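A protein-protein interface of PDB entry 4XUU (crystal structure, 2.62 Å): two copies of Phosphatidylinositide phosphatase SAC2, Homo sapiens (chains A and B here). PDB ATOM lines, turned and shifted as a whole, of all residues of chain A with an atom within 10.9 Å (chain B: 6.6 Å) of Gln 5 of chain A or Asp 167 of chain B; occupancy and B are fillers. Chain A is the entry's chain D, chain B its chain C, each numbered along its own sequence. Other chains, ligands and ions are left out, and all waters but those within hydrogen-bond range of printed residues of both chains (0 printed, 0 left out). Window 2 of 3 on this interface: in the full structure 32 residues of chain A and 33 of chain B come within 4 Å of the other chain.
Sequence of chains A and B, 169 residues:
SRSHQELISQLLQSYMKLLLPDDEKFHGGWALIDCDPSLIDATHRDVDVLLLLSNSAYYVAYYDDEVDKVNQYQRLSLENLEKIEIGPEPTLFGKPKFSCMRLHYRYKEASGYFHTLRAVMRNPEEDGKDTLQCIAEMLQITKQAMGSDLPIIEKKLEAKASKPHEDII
The backbone NH (N) of Tyr 73 of chain B is in hydrogen-bond range of the side-chain carboxylate (OD1) of Asp 167 of chain B, 3.1 Å away. O of Gln 5 of chain A sits at hydrogen-bond distance from OG of Ser 9 of chain A (2.6 Å).
Ile 169 of chain B touches His 4 of chain A (CG2 to CE1, 3.3 Å). Gln 5 of chain A touches Asp 167 of chain B (CG to CB, 3.5 Å). Gln 5 of chain A touches Ile 169 of chain B (NE2 to CG1, 3.4 Å). Ile 8 of chain A touches Tyr 73 of chain B. OG of Ser 9 of chain A touches CG1 of Val 70 of chain B, 3.5 Å away. CD1 of Leu 12 of chain A touches CD2 of Tyr 73 of chain B, 3.7 Å away.
Of the printed residues of chain B, Gln 5 of chain A touches Asp 167 (3.5 Å) and Ile 169 (3.4 Å). Of the printed residues of chain A, Asp 167 of chain B touches Gln 5 (3.5 Å). No residue of chain A comes within 4 Å of Gln 72 of chain B. No residue of chain A comes within 4 Å of Glu 166 of chain B. No residue of chain A comes within 4 Å of Ile 168 of chain B. Of the printed residues of chain A, Ile 169 of chain B touches His 4 (3.3 Å) and Gln 5 (3.4 Å). Printed residues of chain B within 4 Å of Leu 12 of chain A: Tyr 73 (3.7 Å). Ser 3 of chain A touches none of the printed residues of chain B. The nearest residue of chain A that does not touch Asp 167 of chain B is Glu 6 of chain A (6.9 Å).
Printed residues of chain A that touch a printed residue of chain B: His 4, Gln 5, Ile 8, Ser 9 and Leu 12. Hydrophobic or aromatic side chains of chain A within 4 Å of the printed part of chain B: His 4, Ile 8 and Leu 12. Of the 12 printed residues of chain B, 4 touch a printed residue of chain A. Hydrophobic or aromatic side chains of chain B that line the printed part of chain A: Val 70, Tyr 73 and Ile 169.
No position is printed for both chains. Of the 6 pairs that touch across the chains among the printed residues, none has its exchanged pair printed and touching as well.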
ATOM      1  N   SER A   1     -35.352 -17.375 -20.091  1.00  0.00           N
ATOM      2  CA  SER A   1     -35.563 -18.663 -20.809  1.00  0.00           C
ATOM      3  C   SER A   1     -34.816 -19.818 -20.136  1.00  0.00           C
ATOM      4  O   SER A   1     -34.101 -19.620 -19.151  1.00  0.00           O
ATOM      5  CB  SER A   1     -35.155 -18.531 -22.280  1.00  0.00           C
ATOM      6  OG  SER A   1     -33.772 -18.253 -22.404  1.00  0.00           O
ATOM      7  N   ARG A   2     -34.995 -21.017 -20.684  1.00  0.00           N
ATOM      8  CA  ARG A   2     -34.430 -22.245 -20.132  1.00  0.00           C
ATOM      9  C   ARG A   2     -32.927 -22.354 -20.398  1.00  0.00           C
ATOM     10  O   ARG A   2     -32.477 -22.217 -21.538  1.00  0.00           O
ATOM     11  CB  ARG A   2     -35.176 -23.449 -20.719  1.00  0.00           C
ATOM     12  CG  ARG A   2     -34.800 -24.804 -20.146  1.00  0.00           C
ATOM     13  CD  ARG A   2     -35.824 -25.869 -20.535  1.00  0.00           C
ATOM     14  NE  ARG A   2     -36.143 -25.842 -21.962  1.00  0.00           N
ATOM     15  CZ  ARG A   2     -36.986 -26.671 -22.570  1.00  0.00           C
ATOM     16  NH1 ARG A   2     -37.611 -27.624 -21.890  1.00  0.00           N
ATOM     17  NH2 ARG A   2     -37.201 -26.552 -23.871  1.00  0.00           N
ATOM     18  N   SER A   3     -32.162 -22.597 -19.336  1.00  0.00           N
ATOM     19  CA  SER A   3     -30.714 -22.772 -19.438  1.00  0.00           C
ATOM     20  C   SER A   3     -30.361 -24.218 -19.779  1.00  0.00           C
ATOM     21  O   SER A   3     -31.217 -25.107 -19.702  1.00  0.00           O
ATOM     22  CB  SER A   3     -30.028 -22.349 -18.136  1.00  0.00           C
ATOM     23  OG  SER A   3     -30.493 -23.117 -17.041  1.00  0.00           O
ATOM     24  N   HIS A   4     -29.103 -24.448 -20.154  1.00  0.00           N
ATOM     25  CA  HIS A   4     -28.632 -25.780 -20.531  1.00  0.00           C
ATOM     26  C   HIS A   4     -28.812 -26.769 -19.385  1.00  0.00           C
ATOM     27  O   HIS A   4     -29.334 -27.869 -19.589  1.00  0.00           O
ATOM     28  CB  HIS A   4     -27.166 -25.741 -20.973  1.00  0.00           C
ATOM     29  CG  HIS A   4     -26.738 -26.939 -21.767  1.00  0.00           C
ATOM     30  ND1 HIS A   4     -25.664 -26.913 -22.629  1.00  0.00           N
ATOM     31  CD2 HIS A   4     -27.247 -28.191 -21.842  1.00  0.00           C
ATOM     32  CE1 HIS A   4     -25.522 -28.101 -23.189  1.00  0.00           C
ATOM     33  NE2 HIS A   4     -26.471 -28.895 -22.728  1.00  0.00           N
ATOM     34  N   GLN A   5     -28.392 -26.367 -18.186  1.00  0.00           N
ATOM     35  CA  GLN A   5     -28.528 -27.201 -16.991  1.00  0.00           C
ATOM     36  C   GLN A   5     -29.985 -27.530 -16.681  1.00  0.00           C
ATOM     37  O   GLN A   5     -30.290 -28.638 -16.245  1.00  0.00           O
ATOM     38  CB  GLN A   5     -27.875 -26.541 -15.778  1.00  0.00           C
ATOM     39  CG  GLN A   5     -26.357 -26.607 -15.775  1.00  0.00           C
ATOM     40  CD  GLN A   5     -25.701 -25.398 -16.426  1.00  0.00           C
ATOM     41  OE1 GLN A   5     -26.339 -24.372 -16.659  1.00  0.00           O
ATOM     42  NE2 GLN A   5     -24.409 -25.513 -16.707  1.00  0.00           N
ATOM     43  N   GLU A   6     -30.871 -26.571 -16.922  1.00  0.00           N
ATOM     44  CA  GLU A   6     -32.297 -26.784 -16.719  1.00  0.00           C
ATOM     45  C   GLU A   6     -32.818 -27.871 -17.653  1.00  0.00           C
ATOM     46  O   GLU A   6     -33.648 -28.693 -17.263  1.00  0.00           O
ATOM     47  CB  GLU A   6     -33.071 -25.483 -16.943  1.00  0.00           C
ATOM     48  CG  GLU A   6     -32.893 -24.457 -15.836  1.00  0.00           C
ATOM     49  CD  GLU A   6     -33.534 -23.124 -16.169  1.00  0.00           C
ATOM     50  OE1 GLU A   6     -34.064 -22.981 -17.289  1.00  0.00           O
ATOM     51  OE2 GLU A   6     -33.508 -22.220 -15.307  1.00  0.00           O
ATOM     52  N   LEU A   7     -32.330 -27.866 -18.890  1.00  0.00           N
ATOM     53  CA  LEU A   7     -32.805 -28.806 -19.908  1.00  0.00           C
ATOM     54  C   LEU A   7     -32.363 -30.241 -19.630  1.00  0.00           C
ATOM     55  O   LEU A   7     -33.166 -31.168 -19.744  1.00  0.00           O
ATOM     56  CB  LEU A   7     -32.380 -28.367 -21.317  1.00  0.00           C
ATOM     57  CG  LEU A   7     -32.865 -29.205 -22.509  1.00  0.00           C
ATOM     58  CD1 LEU A   7     -34.387 -29.294 -22.566  1.00  0.00           C
ATOM     59  CD2 LEU A   7     -32.318 -28.652 -23.808  1.00  0.00           C
ATOM     60  N   ILE A   8     -31.090 -30.420 -19.269  1.00  0.00           N
ATOM     61  CA  ILE A   8     -30.562 -31.741 -18.910  1.00  0.00           C
ATOM     62  C   ILE A   8     -31.279 -32.273 -17.667  1.00  0.00           C
ATOM     63  O   ILE A   8     -31.513 -33.479 -17.542  1.00  0.00           O
ATOM     64  CB  ILE A   8     -29.028 -31.727 -18.656  1.00  0.00           C
ATOM     65  CG1 ILE A   8     -28.295 -30.923 -19.732  1.00  0.00           C
ATOM     66  CG2 ILE A   8     -28.475 -33.151 -18.612  1.00  0.00           C
ATOM     67  CD1 ILE A   8     -26.862 -30.559 -19.376  1.00  0.00           C
ATOM     68  N   SER A   9     -31.630 -31.353 -16.766  1.00  0.00           N
ATOM     69  CA  SER A   9     -32.348 -31.671 -15.531  1.00  0.00           C
ATOM     70  C   SER A   9     -33.723 -32.282 -15.790  1.00  0.00           C
ATOM     71  O   SER A   9     -34.090 -33.283 -15.170  1.00  0.00           O
ATOM     72  CB  SER A   9     -32.495 -30.418 -14.669  1.00  0.00           C
ATOM     73  OG  SER A   9     -31.230 -29.952 -14.231  1.00  0.00           O
ATOM     74  N   GLN A  10     -34.475 -31.674 -16.706  1.00  0.00           N
ATOM     75  CA  GLN A  10     -35.808 -32.157 -17.068  1.00  0.00           C
ATOM     76  C   GLN A  10     -35.744 -33.383 -17.973  1.00  0.00           C
ATOM     77  O   GLN A  10     -36.706 -34.150 -18.058  1.00  0.00           O
ATOM     78  CB  GLN A  10     -36.628 -31.047 -17.728  1.00  0.00           C
ATOM     79  CG  GLN A  10     -37.076 -29.960 -16.764  1.00  0.00           C
ATOM     80  CD  GLN A  10     -38.059 -28.986 -17.385  1.00  0.00           C
ATOM     81  OE1 GLN A  10     -37.769 -27.798 -17.519  1.00  0.00           O
ATOM     82  NE2 GLN A  10     -39.228 -29.485 -17.772  1.00  0.00           N
ATOM     83  N   LEU A  11     -34.610 -33.555 -18.648  1.00  0.00           N
ATOM     84  CA  LEU A  11     -34.369 -34.728 -19.473  1.00  0.00           C
ATOM     85  C   LEU A  11     -34.108 -35.937 -18.580  1.00  0.00           C
ATOM     86  O   LEU A  11     -34.664 -37.012 -18.809  1.00  0.00           O
ATOM     87  CB  LEU A  11     -33.186 -34.488 -20.413  1.00  0.00           C
ATOM     88  CG  LEU A  11     -33.151 -35.272 -21.728  1.00  0.00           C
ATOM     89  CD1 LEU A  11     -32.392 -34.484 -22.772  1.00  0.00           C
ATOM     90  CD2 LEU A  11     -32.545 -36.660 -21.561  1.00  0.00           C
ATOM     91  N   LEU A  12     -33.264 -35.748 -17.565  1.00  0.00           N
ATOM     92  CA  LEU A  12     -32.988 -36.778 -16.562  1.00  0.00           C
ATOM     93  C   LEU A  12     -34.241 -37.155 -15.775  1.00  0.00           C
ATOM     94  O   LEU A  12     -34.493 -38.336 -15.531  1.00  0.00           O
ATOM     95  CB  LEU A  12     -31.889 -36.319 -15.598  1.00  0.00           C
ATOM     96  CG  LEU A  12     -30.428 -36.613 -15.949  1.00  0.00           C
ATOM     97  CD1 LEU A  12     -29.501 -35.796 -15.071  1.00  0.00           C
ATOM     98  CD2 LEU A  12     -30.113 -38.093 -15.811  1.00  0.00           C
ATOM     99  N   GLN A  13     -35.017 -36.142 -15.393  1.00  0.00           N
ATOM    100  CA  GLN A  13     -36.244 -36.328 -14.620  1.00  0.00           C
ATOM    101  C   GLN A  13     -37.268 -37.200 -15.350  1.00  0.00           C
ATOM    102  O   GLN A  13     -37.690 -38.234 -14.829  1.00  0.00           O
ATOM    103  CB  GLN A  13     -36.861 -34.969 -14.277  1.00  0.00           C
ATOM    104  CG  GLN A  13     -38.175 -35.042 -13.511  1.00  0.00           C
ATOM    105  CD  GLN A  13     -39.017 -33.789 -13.673  1.00  0.00           C
ATOM    106  OE1 GLN A  13     -39.228 -33.042 -12.717  1.00  0.00           O
ATOM    107  NE2 GLN A  13     -39.496 -33.549 -14.891  1.00  0.00           N
ATOM    108  N   VAL B  70     -34.362 -32.221 -10.830  1.00  0.00           N
ATOM    109  CA  VAL B  70     -32.940 -31.965 -10.594  1.00  0.00           C
ATOM    110  C   VAL B  70     -32.735 -30.454 -10.472  1.00  0.00           C
ATOM    111  O   VAL B  70     -33.291 -29.689 -11.262  1.00  0.00           O
ATOM    112  CB  VAL B  70     -32.067 -32.523 -11.757  1.00  0.00           C
ATOM    113  CG1 VAL B  70     -30.605 -32.111 -11.609  1.00  0.00           C
ATOM    114  CG2 VAL B  70     -32.183 -34.040 -11.853  1.00  0.00           C
ATOM    115  N   ASN B  71     -31.945 -30.023  -9.490  1.00  0.00           N
ATOM    116  CA  ASN B  71     -31.658 -28.596  -9.318  1.00  0.00           C
ATOM    117  C   ASN B  71     -30.171 -28.225  -9.400  1.00  0.00           C
ATOM    118  O   ASN B  71     -29.813 -27.046  -9.345  1.00  0.00           O
ATOM    119  CB  ASN B  71     -32.306 -28.055  -8.033  1.00  0.00           C
ATOM    120  CG  ASN B  71     -31.615 -28.536  -6.766  1.00  0.00           C
ATOM    121  OD1 ASN B  71     -31.029 -29.621  -6.723  1.00  0.00           O
ATOM    122  ND2 ASN B  71     -31.695 -27.726  -5.718  1.00  0.00           N
ATOM    123  N   GLN B  72     -29.322 -29.243  -9.529  1.00  0.00           N
ATOM    124  CA  GLN B  72     -27.884 -29.073  -9.737  1.00  0.00           C
ATOM    125  C   GLN B  72     -27.345 -30.269 -10.524  1.00  0.00           C
ATOM    126  O   GLN B  72     -27.653 -31.419 -10.205  1.00  0.00           O
ATOM    127  CB  GLN B  72     -27.151 -28.923  -8.396  1.00  0.00           C
ATOM    128  CG  GLN B  72     -25.634 -28.762  -8.512  1.00  0.00           C
ATOM    129  CD  GLN B  72     -24.946 -28.601  -7.164  1.00  0.00           C
ATOM    130  OE1 GLN B  72     -25.132 -27.598  -6.476  1.00  0.00           O
ATOM    131  NE2 GLN B  72     -24.136 -29.587  -6.789  1.00  0.00           N
ATOM    132  N   TYR B  73     -26.545 -29.987 -11.551  1.00  0.00           N
ATOM    133  CA  TYR B  73     -26.020 -31.020 -12.446  1.00  0.00           C
ATOM    134  C   TYR B  73     -24.589 -30.709 -12.884  1.00  0.00           C
ATOM    135  O   TYR B  73     -24.284 -29.578 -13.273  1.00  0.00           O
ATOM    136  CB  TYR B  73     -26.935 -31.169 -13.668  1.00  0.00           C
ATOM    137  CG  TYR B  73     -26.378 -32.033 -14.780  1.00  0.00           C
ATOM    138  CD1 TYR B  73     -25.501 -31.503 -15.730  1.00  0.00           C
ATOM    139  CD2 TYR B  73     -26.736 -33.373 -14.890  1.00  0.00           C
ATOM    140  CE1 TYR B  73     -24.986 -32.289 -16.754  1.00  0.00           C
ATOM    141  CE2 TYR B  73     -26.228 -34.171 -15.912  1.00  0.00           C
ATOM    142  CZ  TYR B  73     -25.356 -33.620 -16.841  1.00  0.00           C
ATOM    143  OH  TYR B  73     -24.852 -34.398 -17.858  1.00  0.00           O
ATOM    144  N   GLN B  74     -23.726 -31.723 -12.834  1.00  0.00           N
ATOM    145  CA  GLN B  74     -22.319 -31.577 -13.212  1.00  0.00           C
ATOM    146  C   GLN B  74     -21.788 -32.760 -14.024  1.00  0.00           C
ATOM    147  O   GLN B  74     -21.934 -33.914 -13.618  1.00  0.00           O
ATOM    148  CB  GLN B  74     -21.448 -31.415 -11.963  1.00  0.00           C
ATOM    149  CG  GLN B  74     -21.504 -30.051 -11.292  1.00  0.00           C
ATOM    150  CD  GLN B  74     -20.654 -29.987 -10.031  1.00  0.00           C
ATOM    151  OE1 GLN B  74     -20.469 -30.987  -9.339  1.00  0.00           O
ATOM    152  NE2 GLN B  74     -20.137 -28.806  -9.727  1.00  0.00           N
ATOM    153  N   ARG B  75     -21.176 -32.467 -15.170  1.00  0.00           N
ATOM    154  CA  ARG B  75     -20.316 -33.440 -15.839  1.00  0.00           C
ATOM    155  C   ARG B  75     -18.876 -33.147 -15.456  1.00  0.00           C
ATOM    156  O   ARG B  75     -18.364 -32.057 -15.718  1.00  0.00           O
ATOM    157  CB  ARG B  75     -20.451 -33.403 -17.364  1.00  0.00           C
ATOM    158  CG  ARG B  75     -19.467 -34.350 -18.058  1.00  0.00           C
ATOM    159  CD  ARG B  75     -19.452 -34.215 -19.569  1.00  0.00           C
ATOM    160  NE  ARG B  75     -18.519 -35.163 -20.181  1.00  0.00           N
ATOM    161  CZ  ARG B  75     -17.221 -34.934 -20.369  1.00  0.00           C
ATOM    162  NH1 ARG B  75     -16.678 -33.781 -19.995  1.00  0.00           N
ATOM    163  NH2 ARG B  75     -16.461 -35.861 -20.931  1.00  0.00           N
ATOM    164  N   TYR B 107     -11.616 -28.271 -10.013  1.00  0.00           N
ATOM    165  CA  TYR B 107     -12.529 -27.407 -10.750  1.00  0.00           C
ATOM    166  C   TYR B 107     -11.803 -26.124 -11.121  1.00  0.00           C
ATOM    167  O   TYR B 107     -11.441 -25.329 -10.247  1.00  0.00           O
ATOM    168  CB  TYR B 107     -13.782 -27.103  -9.922  1.00  0.00           C
ATOM    169  CG  TYR B 107     -14.742 -26.129 -10.573  1.00  0.00           C
ATOM    170  CD1 TYR B 107     -15.551 -26.521 -11.634  1.00  0.00           C
ATOM    171  CD2 TYR B 107     -14.838 -24.811 -10.127  1.00  0.00           C
ATOM    172  CE1 TYR B 107     -16.434 -25.628 -12.236  1.00  0.00           C
ATOM    173  CE2 TYR B 107     -15.718 -23.910 -10.724  1.00  0.00           C
ATOM    174  CZ  TYR B 107     -16.512 -24.327 -11.776  1.00  0.00           C
ATOM    175  OH  TYR B 107     -17.385 -23.450 -12.371  1.00  0.00           O
ATOM    176  N   HIS B 165     -20.454 -25.520  -5.109  1.00  0.00           N
ATOM    177  CA  HIS B 165     -20.545 -26.234  -6.376  1.00  0.00           C
ATOM    178  C   HIS B 165     -21.121 -25.350  -7.474  1.00  0.00           C
ATOM    179  O   HIS B 165     -22.103 -24.636  -7.263  1.00  0.00           O
ATOM    180  CB  HIS B 165     -21.399 -27.493  -6.228  1.00  0.00           C
ATOM    181  CG  HIS B 165     -20.825 -28.506  -5.287  1.00  0.00           C
ATOM    182  ND1 HIS B 165     -19.590 -29.085  -5.481  1.00  0.00           N
ATOM    183  CD2 HIS B 165     -21.324 -29.050  -4.152  1.00  0.00           C
ATOM    184  CE1 HIS B 165     -19.349 -29.939  -4.501  1.00  0.00           C
ATOM    185  NE2 HIS B 165     -20.385 -29.936  -3.682  1.00  0.00           N
ATOM    186  N   GLU B 166     -20.489 -25.397  -8.643  1.00  0.00           N
ATOM    187  CA  GLU B 166     -20.957 -24.658  -9.811  1.00  0.00           C
ATOM    188  C   GLU B 166     -21.220 -25.617 -10.965  1.00  0.00           C
ATOM    189  O   GLU B 166     -20.518 -26.617 -11.127  1.00  0.00           O
ATOM    190  CB  GLU B 166     -19.954 -23.573 -10.208  1.00  0.00           C
ATOM    191  CG  GLU B 166     -19.859 -22.426  -9.200  1.00  0.00           C
ATOM    192  CD  GLU B 166     -19.013 -21.259  -9.688  1.00  0.00           C
ATOM    193  OE1 GLU B 166     -17.886 -21.490 -10.178  1.00  0.00           O
ATOM    194  OE2 GLU B 166     -19.472 -20.104  -9.568  1.00  0.00           O
ATOM    195  N   ASP B 167     -22.237 -25.305 -11.762  1.00  0.00           N
ATOM    196  CA  ASP B 167     -22.715 -26.217 -12.800  1.00  0.00           C
ATOM    197  C   ASP B 167     -21.777 -26.336 -14.004  1.00  0.00           C
ATOM    198  O   ASP B 167     -21.232 -25.338 -14.485  1.00  0.00           O
ATOM    199  CB  ASP B 167     -24.125 -25.821 -13.241  1.00  0.00           C
ATOM    200  CG  ASP B 167     -25.191 -26.213 -12.225  1.00  0.00           C
ATOM    201  OD1 ASP B 167     -25.083 -27.306 -11.623  1.00  0.00           O
ATOM    202  OD2 ASP B 167     -26.145 -25.428 -12.035  1.00  0.00           O
ATOM    203  N   ILE B 168     -21.595 -27.572 -14.470  1.00  0.00           N
ATOM    204  CA  ILE B 168     -20.719 -27.881 -15.602  1.00  0.00           C
ATOM    205  C   ILE B 168     -21.443 -28.748 -16.628  1.00  0.00           C
ATOM    206  O   ILE B 168     -22.083 -29.741 -16.274  1.00  0.00           O
ATOM    207  CB  ILE B 168     -19.429 -28.627 -15.158  1.00  0.00           C
ATOM    208  CG1 ILE B 168     -18.739 -27.897 -14.004  1.00  0.00           C
ATOM    209  CG2 ILE B 168     -18.466 -28.794 -16.336  1.00  0.00           C
ATOM    210  CD1 ILE B 168     -17.733 -28.742 -13.270  1.00  0.00           C
ATOM    211  N   ILE B 169     -21.321 -28.368 -17.897  1.00  0.00           N
ATOM    212  CA  ILE B 169     -21.877 -29.135 -19.010  1.00  0.00           C
ATOM    213  C   ILE B 169     -20.812 -30.058 -19.607  1.00  0.00           C
ATOM    214  O   ILE B 169     -19.707 -29.636 -19.947  1.00  0.00           O
ATOM    215  CB  ILE B 169     -22.429 -28.213 -20.116  1.00  0.00           C
ATOM    216  CG1 ILE B 169     -23.426 -27.209 -19.528  1.00  0.00           C
ATOM    217  CG2 ILE B 169     -23.088 -29.040 -21.212  1.00  0.00           C
ATOM    218  CD1 ILE B 169     -23.446 -25.870 -20.235  1.00  0.00           C
ATOM    219  OXT ILE B 169     -21.034 -31.257 -19.769  1.00  0.00           O
